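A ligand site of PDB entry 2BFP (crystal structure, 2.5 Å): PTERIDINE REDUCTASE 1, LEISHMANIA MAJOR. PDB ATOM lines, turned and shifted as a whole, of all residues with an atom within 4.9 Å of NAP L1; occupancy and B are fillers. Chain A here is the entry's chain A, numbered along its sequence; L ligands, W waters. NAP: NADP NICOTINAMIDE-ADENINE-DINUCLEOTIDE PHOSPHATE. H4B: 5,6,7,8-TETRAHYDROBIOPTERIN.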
ATOM      1  N   GLY A  13     -17.472  14.015  28.703  1.00  0.00           N
ATOM      2  CA  GLY A  13     -17.911  13.771  27.332  1.00  0.00           C
ATOM      3  C   GLY A  13     -17.639  12.335  26.952  1.00  0.00           C
ATOM      4  O   GLY A  13     -17.101  12.033  25.880  1.00  0.00           O
ATOM      5  N   ALA A  15     -19.882   9.851  26.418  1.00  0.00           N
ATOM      6  CA  ALA A  15     -20.975   9.161  25.731  1.00  0.00           C
ATOM      7  C   ALA A  15     -20.665   8.525  24.386  1.00  0.00           C
ATOM      8  O   ALA A  15     -21.184   7.466  24.056  1.00  0.00           O
ATOM      9  CB  ALA A  15     -22.195  10.060  25.600  1.00  0.00           C
ATOM     10  N   LYS A  16     -19.824   9.169  23.587  1.00  0.00           N
ATOM     11  CA  LYS A  16     -19.521   8.618  22.280  1.00  0.00           C
ATOM     12  C   LYS A  16     -18.102   8.917  21.822  1.00  0.00           C
ATOM     13  O   LYS A  16     -17.306   9.467  22.560  1.00  0.00           O
ATOM     14  CB  LYS A  16     -20.533   9.128  21.241  1.00  0.00           C
ATOM     15  CG  LYS A  16     -21.003  10.564  21.410  1.00  0.00           C
ATOM     16  CD  LYS A  16     -22.387  10.756  20.797  1.00  0.00           C
ATOM     17  CE  LYS A  16     -22.635  12.183  20.331  1.00  0.00           C
ATOM     18  NZ  LYS A  16     -24.104  12.465  20.453  1.00  0.00           N
ATOM     19  N   ARG A  17     -17.791   8.482  20.605  1.00  0.00           N
ATOM     20  CA  ARG A  17     -16.514   8.735  19.949  1.00  0.00           C
ATOM     21  C   ARG A  17     -15.270   8.484  20.810  1.00  0.00           C
ATOM     22  O   ARG A  17     -15.161   7.408  21.416  1.00  0.00           O
ATOM     23  CB  ARG A  17     -16.542  10.118  19.280  1.00  0.00           C
ATOM     24  CG  ARG A  17     -17.540  10.162  18.116  1.00  0.00           C
ATOM     25  CD  ARG A  17     -18.069  11.522  17.744  1.00  0.00           C
ATOM     26  NE  ARG A  17     -16.980  12.416  17.370  1.00  0.00           N
ATOM     27  CZ  ARG A  17     -16.306  12.337  16.230  1.00  0.00           C
ATOM     28  NH1 ARG A  17     -16.619  11.409  15.332  1.00  0.00           N
ATOM     29  NH2 ARG A  17     -15.303  13.171  15.985  1.00  0.00           N
ATOM     30  N   LEU A  18     -14.337   9.434  20.880  1.00  0.00           N
ATOM     31  CA  LEU A  18     -13.100   9.282  21.651  1.00  0.00           C
ATOM     32  C   LEU A  18     -13.354   9.055  23.138  1.00  0.00           C
ATOM     33  O   LEU A  18     -12.774   8.149  23.743  1.00  0.00           O
ATOM     34  CB  LEU A  18     -12.115  10.430  21.406  1.00  0.00           C
ATOM     35  CG  LEU A  18     -11.553  10.696  19.995  1.00  0.00           C
ATOM     36  CD1 LEU A  18     -10.183  11.413  20.004  1.00  0.00           C
ATOM     37  CD2 LEU A  18     -11.469   9.477  19.108  1.00  0.00           C
ATOM     38  N   GLY A  19     -14.220   9.861  23.745  1.00  0.00           N
ATOM     39  CA  GLY A  19     -14.563   9.702  25.149  1.00  0.00           C
ATOM     40  C   GLY A  19     -15.087   8.313  25.478  1.00  0.00           C
ATOM     41  O   GLY A  19     -14.697   7.722  26.491  1.00  0.00           O
ATOM     42  N   HIS A  36     -19.289  11.129  32.311  1.00  0.00           N
ATOM     43  CA  HIS A  36     -19.970  12.414  32.307  1.00  0.00           C
ATOM     44  C   HIS A  36     -20.543  12.676  30.909  1.00  0.00           C
ATOM     45  O   HIS A  36     -19.985  12.262  29.912  1.00  0.00           O
ATOM     46  CB  HIS A  36     -19.020  13.554  32.712  1.00  0.00           C
ATOM     47  CG  HIS A  36     -19.443  14.893  32.201  1.00  0.00           C
ATOM     48  ND1 HIS A  36     -19.206  15.320  30.908  1.00  0.00           N
ATOM     49  CD2 HIS A  36     -20.164  15.885  32.795  1.00  0.00           C
ATOM     50  CE1 HIS A  36     -19.742  16.512  30.739  1.00  0.00           C
ATOM     51  NE2 HIS A  36     -20.313  16.893  31.870  1.00  0.00           N
ATOM     52  N   TYR A  37     -21.649  13.397  30.865  1.00  0.00           N
ATOM     53  CA  TYR A  37     -22.268  13.748  29.595  1.00  0.00           C
ATOM     54  C   TYR A  37     -23.038  15.046  29.777  1.00  0.00           C
ATOM     55  O   TYR A  37     -23.341  15.471  30.888  1.00  0.00           O
ATOM     56  CB  TYR A  37     -23.231  12.645  29.152  1.00  0.00           C
ATOM     57  CG  TYR A  37     -24.473  12.573  30.002  1.00  0.00           C
ATOM     58  CD1 TYR A  37     -24.495  11.884  31.161  1.00  0.00           C
ATOM     59  CD2 TYR A  37     -25.615  13.229  29.700  1.00  0.00           C
ATOM     60  CE1 TYR A  37     -25.614  11.822  31.962  1.00  0.00           C
ATOM     61  CE2 TYR A  37     -26.743  13.138  30.510  1.00  0.00           C
ATOM     62  CZ  TYR A  37     -26.736  12.430  31.646  1.00  0.00           C
ATOM     63  OH  TYR A  37     -27.818  12.336  32.480  1.00  0.00           O
ATOM     64  N   HIS A  38     -23.328  15.701  28.663  1.00  0.00           N
ATOM     65  CA  HIS A  38     -24.068  16.958  28.714  1.00  0.00           C
ATOM     66  C   HIS A  38     -25.425  16.719  28.052  1.00  0.00           C
ATOM     67  O   HIS A  38     -26.442  16.667  28.727  1.00  0.00           O
ATOM     68  CB  HIS A  38     -23.275  18.079  28.031  1.00  0.00           C
ATOM     69  CG  HIS A  38     -23.992  19.400  28.019  1.00  0.00           C
ATOM     70  ND1 HIS A  38     -23.916  20.276  26.960  1.00  0.00           N
ATOM     71  CD2 HIS A  38     -24.830  19.963  28.926  1.00  0.00           C
ATOM     72  CE1 HIS A  38     -24.676  21.332  27.215  1.00  0.00           C
ATOM     73  NE2 HIS A  38     -25.218  21.173  28.408  1.00  0.00           N
ATOM     74  N   ARG A  39     -25.427  16.490  26.749  1.00  0.00           N
ATOM     75  CA  ARG A  39     -26.674  16.260  26.034  1.00  0.00           C
ATOM     76  C   ARG A  39     -26.928  14.814  25.591  1.00  0.00           C
ATOM     77  O   ARG A  39     -28.033  14.480  25.194  1.00  0.00           O
ATOM     78  CB  ARG A  39     -26.774  17.231  24.857  1.00  0.00           C
ATOM     79  CG  ARG A  39     -27.003  18.679  25.321  1.00  0.00           C
ATOM     80  CD  ARG A  39     -26.814  19.712  24.233  1.00  0.00           C
ATOM     81  NE  ARG A  39     -26.712  21.077  24.756  1.00  0.00           N
ATOM     82  CZ  ARG A  39     -26.035  22.057  24.162  1.00  0.00           C
ATOM     83  NH1 ARG A  39     -25.402  21.851  23.001  1.00  0.00           N
ATOM     84  NH2 ARG A  39     -26.006  23.268  24.727  1.00  0.00           N
ATOM     85  N   SER A  40     -25.953  13.934  25.731  1.00  0.00           N
ATOM     86  CA  SER A  40     -26.122  12.577  25.261  1.00  0.00           C
ATOM     87  C   SER A  40     -26.505  11.577  26.356  1.00  0.00           C
ATOM     88  O   SER A  40     -25.805  10.582  26.572  1.00  0.00           O
ATOM     89  CB  SER A  40     -24.854  12.116  24.538  1.00  0.00           C
ATOM     90  OG  SER A  40     -24.666  12.824  23.337  1.00  0.00           O
ATOM     91  N   ALA A  64     -23.648  17.259  33.165  1.00  0.00           N
ATOM     92  CA  ALA A  64     -23.179  18.603  33.479  1.00  0.00           C
ATOM     93  C   ALA A  64     -22.810  19.438  32.272  1.00  0.00           C
ATOM     94  O   ALA A  64     -22.134  18.974  31.354  1.00  0.00           O
ATOM     95  CB  ALA A  64     -22.043  18.605  34.485  1.00  0.00           C
ATOM     96  N   ASP A  65     -23.321  20.652  32.272  1.00  0.00           N
ATOM     97  CA  ASP A  65     -22.977  21.632  31.267  1.00  0.00           C
ATOM     98  C   ASP A  65     -21.644  22.168  31.770  1.00  0.00           C
ATOM     99  O   ASP A  65     -21.568  22.681  32.882  1.00  0.00           O
ATOM    100  CB  ASP A  65     -24.004  22.744  31.234  1.00  0.00           C
ATOM    101  CG  ASP A  65     -23.759  23.719  30.087  1.00  0.00           C
ATOM    102  OD1 ASP A  65     -22.666  23.641  29.472  1.00  0.00           O
ATOM    103  OD2 ASP A  65     -24.627  24.551  29.729  1.00  0.00           O
ATOM    104  N   LEU A  66     -20.587  22.027  30.975  1.00  0.00           N
ATOM    105  CA  LEU A  66     -19.260  22.487  31.378  1.00  0.00           C
ATOM    106  C   LEU A  66     -18.949  23.845  30.785  1.00  0.00           C
ATOM    107  O   LEU A  66     -17.799  24.295  30.796  1.00  0.00           O
ATOM    108  CB  LEU A  66     -18.198  21.455  30.986  1.00  0.00           C
ATOM    109  CG  LEU A  66     -18.362  20.117  31.681  1.00  0.00           C
ATOM    110  CD1 LEU A  66     -17.275  19.102  31.303  1.00  0.00           C
ATOM    111  CD2 LEU A  66     -18.422  20.327  33.183  1.00  0.00           C
ATOM    112  N   SER A  67     -19.961  24.488  30.230  1.00  0.00           N
ATOM    113  CA  SER A  67     -19.816  25.814  29.661  1.00  0.00           C
ATOM    114  C   SER A  67     -19.617  26.777  30.828  1.00  0.00           C
ATOM    115  O   SER A  67     -20.155  26.547  31.912  1.00  0.00           O
ATOM    116  CB  SER A  67     -21.047  26.163  28.844  1.00  0.00           C
ATOM    117  OG  SER A  67     -21.028  27.532  28.535  1.00  0.00           O
ATOM    118  N   ASN A 109     -11.923  15.411  28.396  1.00  0.00           N
ATOM    119  CA  ASN A 109     -12.188  15.084  26.992  1.00  0.00           C
ATOM    120  C   ASN A 109     -13.324  15.903  26.385  1.00  0.00           C
ATOM    121  O   ASN A 109     -13.275  16.213  25.203  1.00  0.00           O
ATOM    122  CB  ASN A 109     -12.452  13.573  26.856  1.00  0.00           C
ATOM    123  CG  ASN A 109     -12.954  13.171  25.467  1.00  0.00           C
ATOM    124  OD1 ASN A 109     -12.175  12.977  24.545  1.00  0.00           O
ATOM    125  ND2 ASN A 109     -14.251  13.008  25.346  1.00  0.00           N
ATOM    126  N   ALA A 110     -14.325  16.246  27.191  1.00  0.00           N
ATOM    127  CA  ALA A 110     -15.482  17.008  26.695  1.00  0.00           C
ATOM    128  C   ALA A 110     -14.986  18.268  26.030  1.00  0.00           C
ATOM    129  O   ALA A 110     -14.070  18.918  26.541  1.00  0.00           O
ATOM    130  CB  ALA A 110     -16.459  17.341  27.808  1.00  0.00           C
ATOM    131  N   SER A 111     -15.599  18.625  24.900  1.00  0.00           N
ATOM    132  CA  SER A 111     -15.134  19.760  24.126  1.00  0.00           C
ATOM    133  C   SER A 111     -16.092  20.204  23.034  1.00  0.00           C
ATOM    134  O   SER A 111     -16.582  19.397  22.229  1.00  0.00           O
ATOM    135  CB  SER A 111     -13.781  19.386  23.483  1.00  0.00           C
ATOM    136  OG  SER A 111     -13.529  20.073  22.263  1.00  0.00           O
ATOM    137  N   SER A 112     -16.398  21.491  23.028  1.00  0.00           N
ATOM    138  CA  SER A 112     -17.224  22.010  21.951  1.00  0.00           C
ATOM    139  C   SER A 112     -16.285  22.477  20.825  1.00  0.00           C
ATOM    140  O   SER A 112     -15.155  22.921  21.065  1.00  0.00           O
ATOM    141  CB  SER A 112     -18.212  23.088  22.413  1.00  0.00           C
ATOM    142  OG  SER A 112     -17.593  24.127  23.124  1.00  0.00           O
ATOM    143  N   ASP A 142     -19.021  28.667  26.086  1.00  0.00           N
ATOM    144  CA  ASP A 142     -19.102  27.266  25.753  1.00  0.00           C
ATOM    145  C   ASP A 142     -17.748  26.717  25.284  1.00  0.00           C
ATOM    146  O   ASP A 142     -17.221  25.745  25.830  1.00  0.00           O
ATOM    147  CB  ASP A 142     -20.149  27.097  24.658  1.00  0.00           C
ATOM    148  CG  ASP A 142     -20.364  25.672  24.256  1.00  0.00           C
ATOM    149  OD1 ASP A 142     -20.426  24.823  25.158  1.00  0.00           O
ATOM    150  OD2 ASP A 142     -20.506  25.292  23.077  1.00  0.00           O
ATOM    151  N   SER A 146     -15.714  24.347  28.117  1.00  0.00           N
ATOM    152  CA  SER A 146     -15.526  22.926  27.852  1.00  0.00           C
ATOM    153  C   SER A 146     -14.066  22.548  27.617  1.00  0.00           C
ATOM    154  O   SER A 146     -13.570  21.586  28.191  1.00  0.00           O
ATOM    155  CB  SER A 146     -16.406  22.476  26.692  1.00  0.00           C
ATOM    156  OG  SER A 146     -15.948  22.959  25.445  1.00  0.00           O
ATOM    157  N   ASN A 147     -13.366  23.338  26.807  1.00  0.00           N
ATOM    158  CA  ASN A 147     -11.990  23.069  26.462  1.00  0.00           C
ATOM    159  C   ASN A 147     -10.946  23.554  27.452  1.00  0.00           C
ATOM    160  O   ASN A 147      -9.830  23.022  27.440  1.00  0.00           O
ATOM    161  CB  ASN A 147     -11.647  23.689  25.085  1.00  0.00           C
ATOM    162  CG  ASN A 147     -12.418  23.059  23.949  1.00  0.00           C
ATOM    163  OD1 ASN A 147     -12.207  21.893  23.622  1.00  0.00           O
ATOM    164  ND2 ASN A 147     -13.341  23.820  23.376  1.00  0.00           N
ATOM    165  N   MET A 179      -7.323  16.375  26.700  1.00  0.00           N
ATOM    166  CA  MET A 179      -7.362  16.107  25.271  1.00  0.00           C
ATOM    167  C   MET A 179      -7.097  17.389  24.512  1.00  0.00           C
ATOM    168  O   MET A 179      -7.937  18.292  24.494  1.00  0.00           O
ATOM    169  CB  MET A 179      -8.684  15.458  24.875  1.00  0.00           C
ATOM    170  CG  MET A 179      -8.952  14.152  25.596  1.00  0.00           C
ATOM    171  SD  MET A 179      -7.725  12.826  25.306  1.00  0.00           S
ATOM    172  CE  MET A 179      -7.865  12.541  23.531  1.00  0.00           C
ATOM    173  N   VAL A 180      -5.879  17.518  24.004  1.00  0.00           N
ATOM    174  CA  VAL A 180      -5.489  18.694  23.258  1.00  0.00           C
ATOM    175  C   VAL A 180      -5.711  18.506  21.763  1.00  0.00           C
ATOM    176  O   VAL A 180      -6.619  17.784  21.366  1.00  0.00           O
ATOM    177  CB  VAL A 180      -4.085  19.191  23.642  1.00  0.00           C
ATOM    178  CG1 VAL A 180      -4.092  19.763  25.069  1.00  0.00           C
ATOM    179  CG2 VAL A 180      -3.045  18.099  23.470  1.00  0.00           C
ATOM    180  N   ASP A 181      -4.913  19.133  20.909  1.00  0.00           N
ATOM    181  CA  ASP A 181      -5.140  19.033  19.475  1.00  0.00           C
ATOM    182  C   ASP A 181      -3.807  19.171  18.766  1.00  0.00           C
ATOM    183  O   ASP A 181      -3.206  20.232  18.801  1.00  0.00           O
ATOM    184  CB  ASP A 181      -6.085  20.138  19.021  1.00  0.00           C
ATOM    185  CG  ASP A 181      -6.424  20.080  17.533  1.00  0.00           C
ATOM    186  OD1 ASP A 181      -5.668  19.511  16.712  1.00  0.00           O
ATOM    187  OD2 ASP A 181      -7.452  20.618  17.073  1.00  0.00           O
ATOM    188  N   TYR A 194     -11.831  28.325  19.569  1.00  0.00           N
ATOM    189  CA  TYR A 194     -11.538  26.925  19.844  1.00  0.00           C
ATOM    190  C   TYR A 194     -10.029  26.704  19.939  1.00  0.00           C
ATOM    191  O   TYR A 194      -9.539  26.053  20.864  1.00  0.00           O
ATOM    192  CB  TYR A 194     -12.105  26.015  18.750  1.00  0.00           C
ATOM    193  CG  TYR A 194     -11.479  24.630  18.753  1.00  0.00           C
ATOM    194  CD1 TYR A 194     -11.946  23.636  19.597  1.00  0.00           C
ATOM    195  CD2 TYR A 194     -10.398  24.340  17.917  1.00  0.00           C
ATOM    196  CE1 TYR A 194     -11.362  22.368  19.603  1.00  0.00           C
ATOM    197  CE2 TYR A 194      -9.811  23.088  17.913  1.00  0.00           C
ATOM    198  CZ  TYR A 194     -10.291  22.103  18.747  1.00  0.00           C
ATOM    199  OH  TYR A 194      -9.706  20.842  18.749  1.00  0.00           O
ATOM    200  N   LYS A 198      -7.728  25.529  23.198  1.00  0.00           N
ATOM    201  CA  LYS A 198      -6.802  24.408  23.251  1.00  0.00           C
ATOM    202  C   LYS A 198      -5.418  24.891  23.683  1.00  0.00           C
ATOM    203  O   LYS A 198      -4.722  24.219  24.454  1.00  0.00           O
ATOM    204  CB  LYS A 198      -6.748  23.631  21.945  1.00  0.00           C
ATOM    205  CG  LYS A 198      -8.022  22.847  21.629  1.00  0.00           C
ATOM    206  CD  LYS A 198      -8.354  21.801  22.702  1.00  0.00           C
ATOM    207  CE  LYS A 198      -9.407  20.852  22.142  1.00  0.00           C
ATOM    208  NZ  LYS A 198      -9.878  19.868  23.130  1.00  0.00           N
ATOM    209  N   PRO A 224      -5.007  14.466  19.282  1.00  0.00           N
ATOM    210  CA  PRO A 224      -5.335  13.827  18.012  1.00  0.00           C
ATOM    211  C   PRO A 224      -5.118  14.801  16.858  1.00  0.00           C
ATOM    212  O   PRO A 224      -4.984  16.012  17.073  1.00  0.00           O
ATOM    213  CB  PRO A 224      -6.832  13.544  18.143  1.00  0.00           C
ATOM    214  CG  PRO A 224      -7.078  13.494  19.608  1.00  0.00           C
ATOM    215  CD  PRO A 224      -6.183  14.571  20.163  1.00  0.00           C
ATOM    216  N   GLY A 225      -5.041  14.251  15.650  1.00  0.00           N
ATOM    217  CA  GLY A 225      -4.899  15.020  14.420  1.00  0.00           C
ATOM    218  C   GLY A 225      -6.281  14.950  13.828  1.00  0.00           C
ATOM    219  O   GLY A 225      -7.106  15.836  14.047  1.00  0.00           O
ATOM    220  N   LEU A 226      -6.542  13.881  13.078  1.00  0.00           N
ATOM    221  CA  LEU A 226      -7.875  13.653  12.513  1.00  0.00           C
ATOM    222  C   LEU A 226      -8.321  12.304  13.033  1.00  0.00           C
ATOM    223  O   LEU A 226      -7.677  11.285  12.771  1.00  0.00           O
ATOM    224  CB  LEU A 226      -7.845  13.647  10.986  1.00  0.00           C
ATOM    225  CG  LEU A 226      -7.442  14.974  10.309  1.00  0.00           C
ATOM    226  CD1 LEU A 226      -7.586  14.888   8.785  1.00  0.00           C
ATOM    227  CD2 LEU A 226      -8.222  16.181  10.851  1.00  0.00           C
ATOM    228  N   SER A 227      -9.358  12.305  13.878  1.00  0.00           N
ATOM    229  CA  SER A 227      -9.873  11.042  14.424  1.00  0.00           C
ATOM    230  C   SER A 227     -11.354  10.862  14.197  1.00  0.00           C
ATOM    231  O   SER A 227     -12.114  11.761  14.524  1.00  0.00           O
ATOM    232  CB  SER A 227      -9.570  10.919  15.901  1.00  0.00           C
ATOM    233  OG  SER A 227      -8.179  10.820  16.064  1.00  0.00           O
ATOM    234  N   VAL A 228     -11.752   9.667  13.740  1.00  0.00           N
ATOM    235  CA  VAL A 228     -13.149   9.345  13.442  1.00  0.00           C
ATOM    236  C   VAL A 228     -13.825  10.561  12.850  1.00  0.00           C
ATOM    237  O   VAL A 228     -14.876  11.020  13.322  1.00  0.00           O
ATOM    238  CB  VAL A 228     -13.912   8.814  14.657  1.00  0.00           C
ATOM    239  CG1 VAL A 228     -13.497   7.377  14.922  1.00  0.00           C
ATOM    240  CG2 VAL A 228     -13.652   9.663  15.885  1.00  0.00           C
HETATM  241  PA  NAP L   1     -16.643  15.262  20.263  1.00  0.00           P
HETATM  242  O1A NAP L   1     -16.616  16.400  19.319  1.00  0.00           O
HETATM  243  O2A NAP L   1     -17.350  14.059  19.648  1.00  0.00           O
HETATM  244  O5B NAP L   1     -17.320  15.703  21.630  1.00  0.00           O
HETATM  245  C5B NAP L   1     -17.070  15.053  22.836  1.00  0.00           C
HETATM  246  C4B NAP L   1     -18.108  15.487  23.868  1.00  0.00           C
HETATM  247  O4B NAP L   1     -17.872  16.754  24.474  1.00  0.00           O
HETATM  248  C3B NAP L   1     -19.498  15.646  23.276  1.00  0.00           C
HETATM  249  O3B NAP L   1     -20.080  14.399  23.012  1.00  0.00           O
HETATM  250  C2B NAP L   1     -20.230  16.447  24.352  1.00  0.00           C
HETATM  251  O2B NAP L   1     -21.030  15.652  25.206  1.00  0.00           O
HETATM  252  C1B NAP L   1     -19.075  17.072  25.139  1.00  0.00           C
HETATM  253  N9A NAP L   1     -19.281  18.516  25.231  1.00  0.00           N
HETATM  254  C8A NAP L   1     -19.245  19.463  24.253  1.00  0.00           C
HETATM  255  N7A NAP L   1     -19.508  20.683  24.785  1.00  0.00           N
HETATM  256  C5A NAP L   1     -19.746  20.502  26.103  1.00  0.00           C
HETATM  257  C6A NAP L   1     -20.070  21.369  27.133  1.00  0.00           C
HETATM  258  N6A NAP L   1     -20.481  22.612  26.904  1.00  0.00           N
HETATM  259  N1A NAP L   1     -20.257  20.851  28.389  1.00  0.00           N
HETATM  260  C2A NAP L   1     -20.128  19.506  28.638  1.00  0.00           C
HETATM  261  N3A NAP L   1     -19.792  18.656  27.618  1.00  0.00           N
HETATM  262  C4A NAP L   1     -19.603  19.152  26.386  1.00  0.00           C
HETATM  263  O3  NAP L   1     -15.113  14.951  20.631  1.00  0.00           O
HETATM  264  PN  NAP L   1     -14.155  13.873  19.885  1.00  0.00           P
HETATM  265  O1N NAP L   1     -14.110  14.153  18.431  1.00  0.00           O
HETATM  266  O2N NAP L   1     -14.461  12.526  20.402  1.00  0.00           O
HETATM  267  O5D NAP L   1     -12.746  14.348  20.515  1.00  0.00           O
HETATM  268  C5D NAP L   1     -12.449  14.146  21.869  1.00  0.00           C
HETATM  269  C4D NAP L   1     -11.355  15.124  22.278  1.00  0.00           C
HETATM  270  O4D NAP L   1     -10.279  15.044  21.358  1.00  0.00           O
HETATM  271  C3D NAP L   1     -11.856  16.559  22.270  1.00  0.00           C
HETATM  272  O3D NAP L   1     -11.234  17.255  23.324  1.00  0.00           O
HETATM  273  C2D NAP L   1     -11.320  17.080  20.950  1.00  0.00           C
HETATM  274  O2D NAP L   1     -11.093  18.462  20.969  1.00  0.00           O
HETATM  275  C1D NAP L   1     -10.010  16.326  20.822  1.00  0.00           C
HETATM  276  N1N NAP L   1      -9.710  16.247  19.392  1.00  0.00           N
HETATM  277  C2N NAP L   1     -10.513  15.527  18.538  1.00  0.00           C
HETATM  278  C3N NAP L   1     -10.213  15.483  17.182  1.00  0.00           C
HETATM  279  C7N NAP L   1     -10.926  14.594  16.215  1.00  0.00           C
HETATM  280  O7N NAP L   1     -10.399  14.529  14.915  1.00  0.00           O
HETATM  281  N7N NAP L   1     -11.994  13.874  16.547  1.00  0.00           N
HETATM  282  C4N NAP L   1      -9.090  16.171  16.738  1.00  0.00           C
HETATM  283  C5N NAP L   1      -8.291  16.899  17.602  1.00  0.00           C
HETATM  284  C6N NAP L   1      -8.611  16.929  18.953  1.00  0.00           C
HETATM  285  P2B NAP L   1     -22.614  15.414  25.014  1.00  0.00           P
HETATM  286  O1X NAP L   1     -23.136  14.544  26.093  1.00  0.00           O
HETATM  287  O2X NAP L   1     -23.415  16.710  25.020  1.00  0.00           O
HETATM  288  O3X NAP L   1     -22.787  14.756  23.637  1.00  0.00           O
HETATM  289  N1  H4B L   2     -12.876  18.832  18.608  1.00  0.00           N
HETATM  290  C2  H4B L   2     -14.061  18.270  18.972  1.00  0.00           C
HETATM  291  N2  H4B L   2     -14.604  18.509  20.148  1.00  0.00           N
HETATM  292  N3  H4B L   2     -14.678  17.460  18.096  1.00  0.00           N
HETATM  293  C4  H4B L   2     -14.187  17.144  16.825  1.00  0.00           C
HETATM  294  O4  H4B L   2     -14.844  16.366  16.118  1.00  0.00           O
HETATM  295  C4A H4B L   2     -12.935  17.761  16.505  1.00  0.00           C
HETATM  296  C8A H4B L   2     -12.291  18.605  17.384  1.00  0.00           C
HETATM  297  N5  H4B L   2     -12.372  17.473  15.183  1.00  0.00           N
HETATM  298  N8  H4B L   2     -11.181  19.272  17.092  1.00  0.00           N
HETATM  299  C6  H4B L   2     -10.957  17.971  14.976  1.00  0.00           C
HETATM  300  C7  H4B L   2     -10.681  19.265  15.726  1.00  0.00           C
HETATM  301  C9  H4B L   2     -10.544  17.919  13.482  1.00  0.00           C
HETATM  302  O9  H4B L   2     -10.737  16.612  12.935  1.00  0.00           O
HETATM  303  C10 H4B L   2     -11.134  18.971  12.525  1.00  0.00           C
HETATM  304  C11 H4B L   2     -12.505  18.736  12.016  1.00  0.00           C
HETATM  305  O10 H4B L   2     -10.236  18.974  11.415  1.00  0.00           O
HETATM  306  O   HOH W   1     -20.653  12.644  26.632  1.00  0.00           O
HETATM  307  O   HOH W   2     -15.680  11.990  22.827  1.00  0.00           O
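Gly 13 touches NAP L1 (CA to C4B, 3.9 Å). His 36 touches NAP L1 (CE1 to C2A, 3.7 Å). CB of Tyr 37 touches O1X of NAP L1, at 3.6 Å. Ala 64 touches NAP L1 (O to C2A, 3.4 Å). OD1 of Asp 65 touches N6A of NAP L1, at 3.5 Å. Ser 67 touches NAP L1 (N to N6A, 3.9 Å). Ala 110 touches NAP L1 (CA to O4B, 3.3 Å). Ser 112 touches NAP L1 (CB to N7A, 3.6 Å). Ser 146 touches NAP L1. Met 179 touches NAP L1 (CB to O3D, 3.5 Å). Val 180 touches NAP L1 (O to C6N, 3.2 Å). Asp 181 touches NAP L1. OH of Tyr 194 touches O2D of NAP L1, at 3.5 Å. O of Pro 224 touches C5N of NAP L1 (3.5 Å). Gly 225 touches NAP L1 (O to C4N, 3.4 Å). Leu 226 touches NAP L1 (C to O7N, 3.6 Å). Hydrophobic or aromatic side chains that line NAP L1: Leu 18, His 36, Tyr 37, His 38, Leu 66, Ala 110, Met 179 and Pro 224. 27 residues have an atom within 4 Å of NAP L1: Gly 13, Arg 17, Leu 18, His 36, Tyr 37, His 38, Arg 39, Ser 40, Ala 64, Asp 65, Leu 66, Ser 67, Asn 109, Ala 110, Ser 111, Ser 112, Asp 142, Ser 146, Met 179, Val 180, Asp 181, Tyr 194, Lys 198, Pro 224, Gly 225, Leu 226 and Ser 227. The nearest printed residue that does not touch NAP L1 is Lys 16 (4.1 Å).
An oxygen (O1A) of NAP L1 sits at hydrogen-bond distance from a nitrogen (N3) of H4B L2, at 2.5 Å.
Water W1 lies within hydrogen-bond range of N of Ala 15, O1X of NAP L1 and O of His 36.
The side-chain hydroxyl (OG) of Ser 112 sits at hydrogen-bond distance from the side-chain carboxylate (OD2) of Asp 142 (3.1 Å). The backbone carbonyl oxygen (O) of Ala 64 is in hydrogen-bond range of a ring nitrogen (NE2) of His 36, at 2.8 Å. NZ of Lys 16 is in hydrogen-bond range of OG of Ser 40. OG of Ser 146 lies within hydrogen-bond range of ND2 of Asn 147 (3.4 Å). NZ of Lys 198 sits at hydrogen-bond distance from O of Met 179, at 2.8 Å. The backbone NH of Ser 146 lies within hydrogen-bond range of the backbone carbonyl oxygen of Leu 66. The backbone NH (N) of Ser 112 sits at hydrogen-bond distance from the side-chain hydroxyl (OG) of Ser 146. The backbone NH (N) of Asp 142 is in hydrogen-bond range of the side-chain hydroxyl (OG) of Ser 67, 3.4 Å away.
An oxygen (O2D) of NAP L1 is in hydrogen-bond range of the side-chain amino group (NZ) of Lys 198. The backbone NH of Leu 18 sits at hydrogen-bond distance from an oxygen (O2N) of NAP L1, 3.1 Å away. An oxygen (O3D) of NAP L1 lies within hydrogen-bond range of the backbone carbonyl oxygen (O) of Asn 109. N2 of H4B L2 sits at hydrogen-bond distance from OG of Ser 111 (2.8 Å). O1X of NAP L1 is in hydrogen-bond range of N of His 38. N7N of NAP L1 is in hydrogen-bond range of O of Ser 227 (2.9 Å). The backbone NH of Arg 39 is in hydrogen-bond range of an oxygen (O2X) of NAP L1 (2.7 Å). An oxygen (O3X) of NAP L1 sits at hydrogen-bond distance from the side-chain hydroxyl (OG) of Ser 40. The backbone carbonyl oxygen (O) of Ser 111 is in hydrogen-bond range of a nitrogen (N2) of H4B L2, 3.0 Å away. NH2 of Arg 17 is in hydrogen-bond range of O4 of H4B L2, 3.2 Å away. An oxygen (O1X) of NAP L1 sits at hydrogen-bond distance from the backbone NH (N) of Ser 40. An oxygen (O2A) of NAP L1 is in salt-bridge range of the guanidinium group of Arg 17 (2.8 Å). The backbone NH of Ser 227 is in hydrogen-bond range of an oxygen (O7N) of NAP L1. The backbone NH of Leu 66 sits at hydrogen-bond distance from a nitrogen (N1A) of NAP L1, at 2.9 Å. N of Ser 111 is in hydrogen-bond range of O4B of NAP L1 (3.0 Å). N8 of H4B L2 lies within hydrogen-bond range of OH of Tyr 194, at 2.7 Å. N6A of NAP L1 is in hydrogen-bond range of OD1 of Asp 142 (2.8 Å). An oxygen (O2D) of NAP L1 is in hydrogen-bond range of the side-chain hydroxyl of Ser 111, at 3.2 Å.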
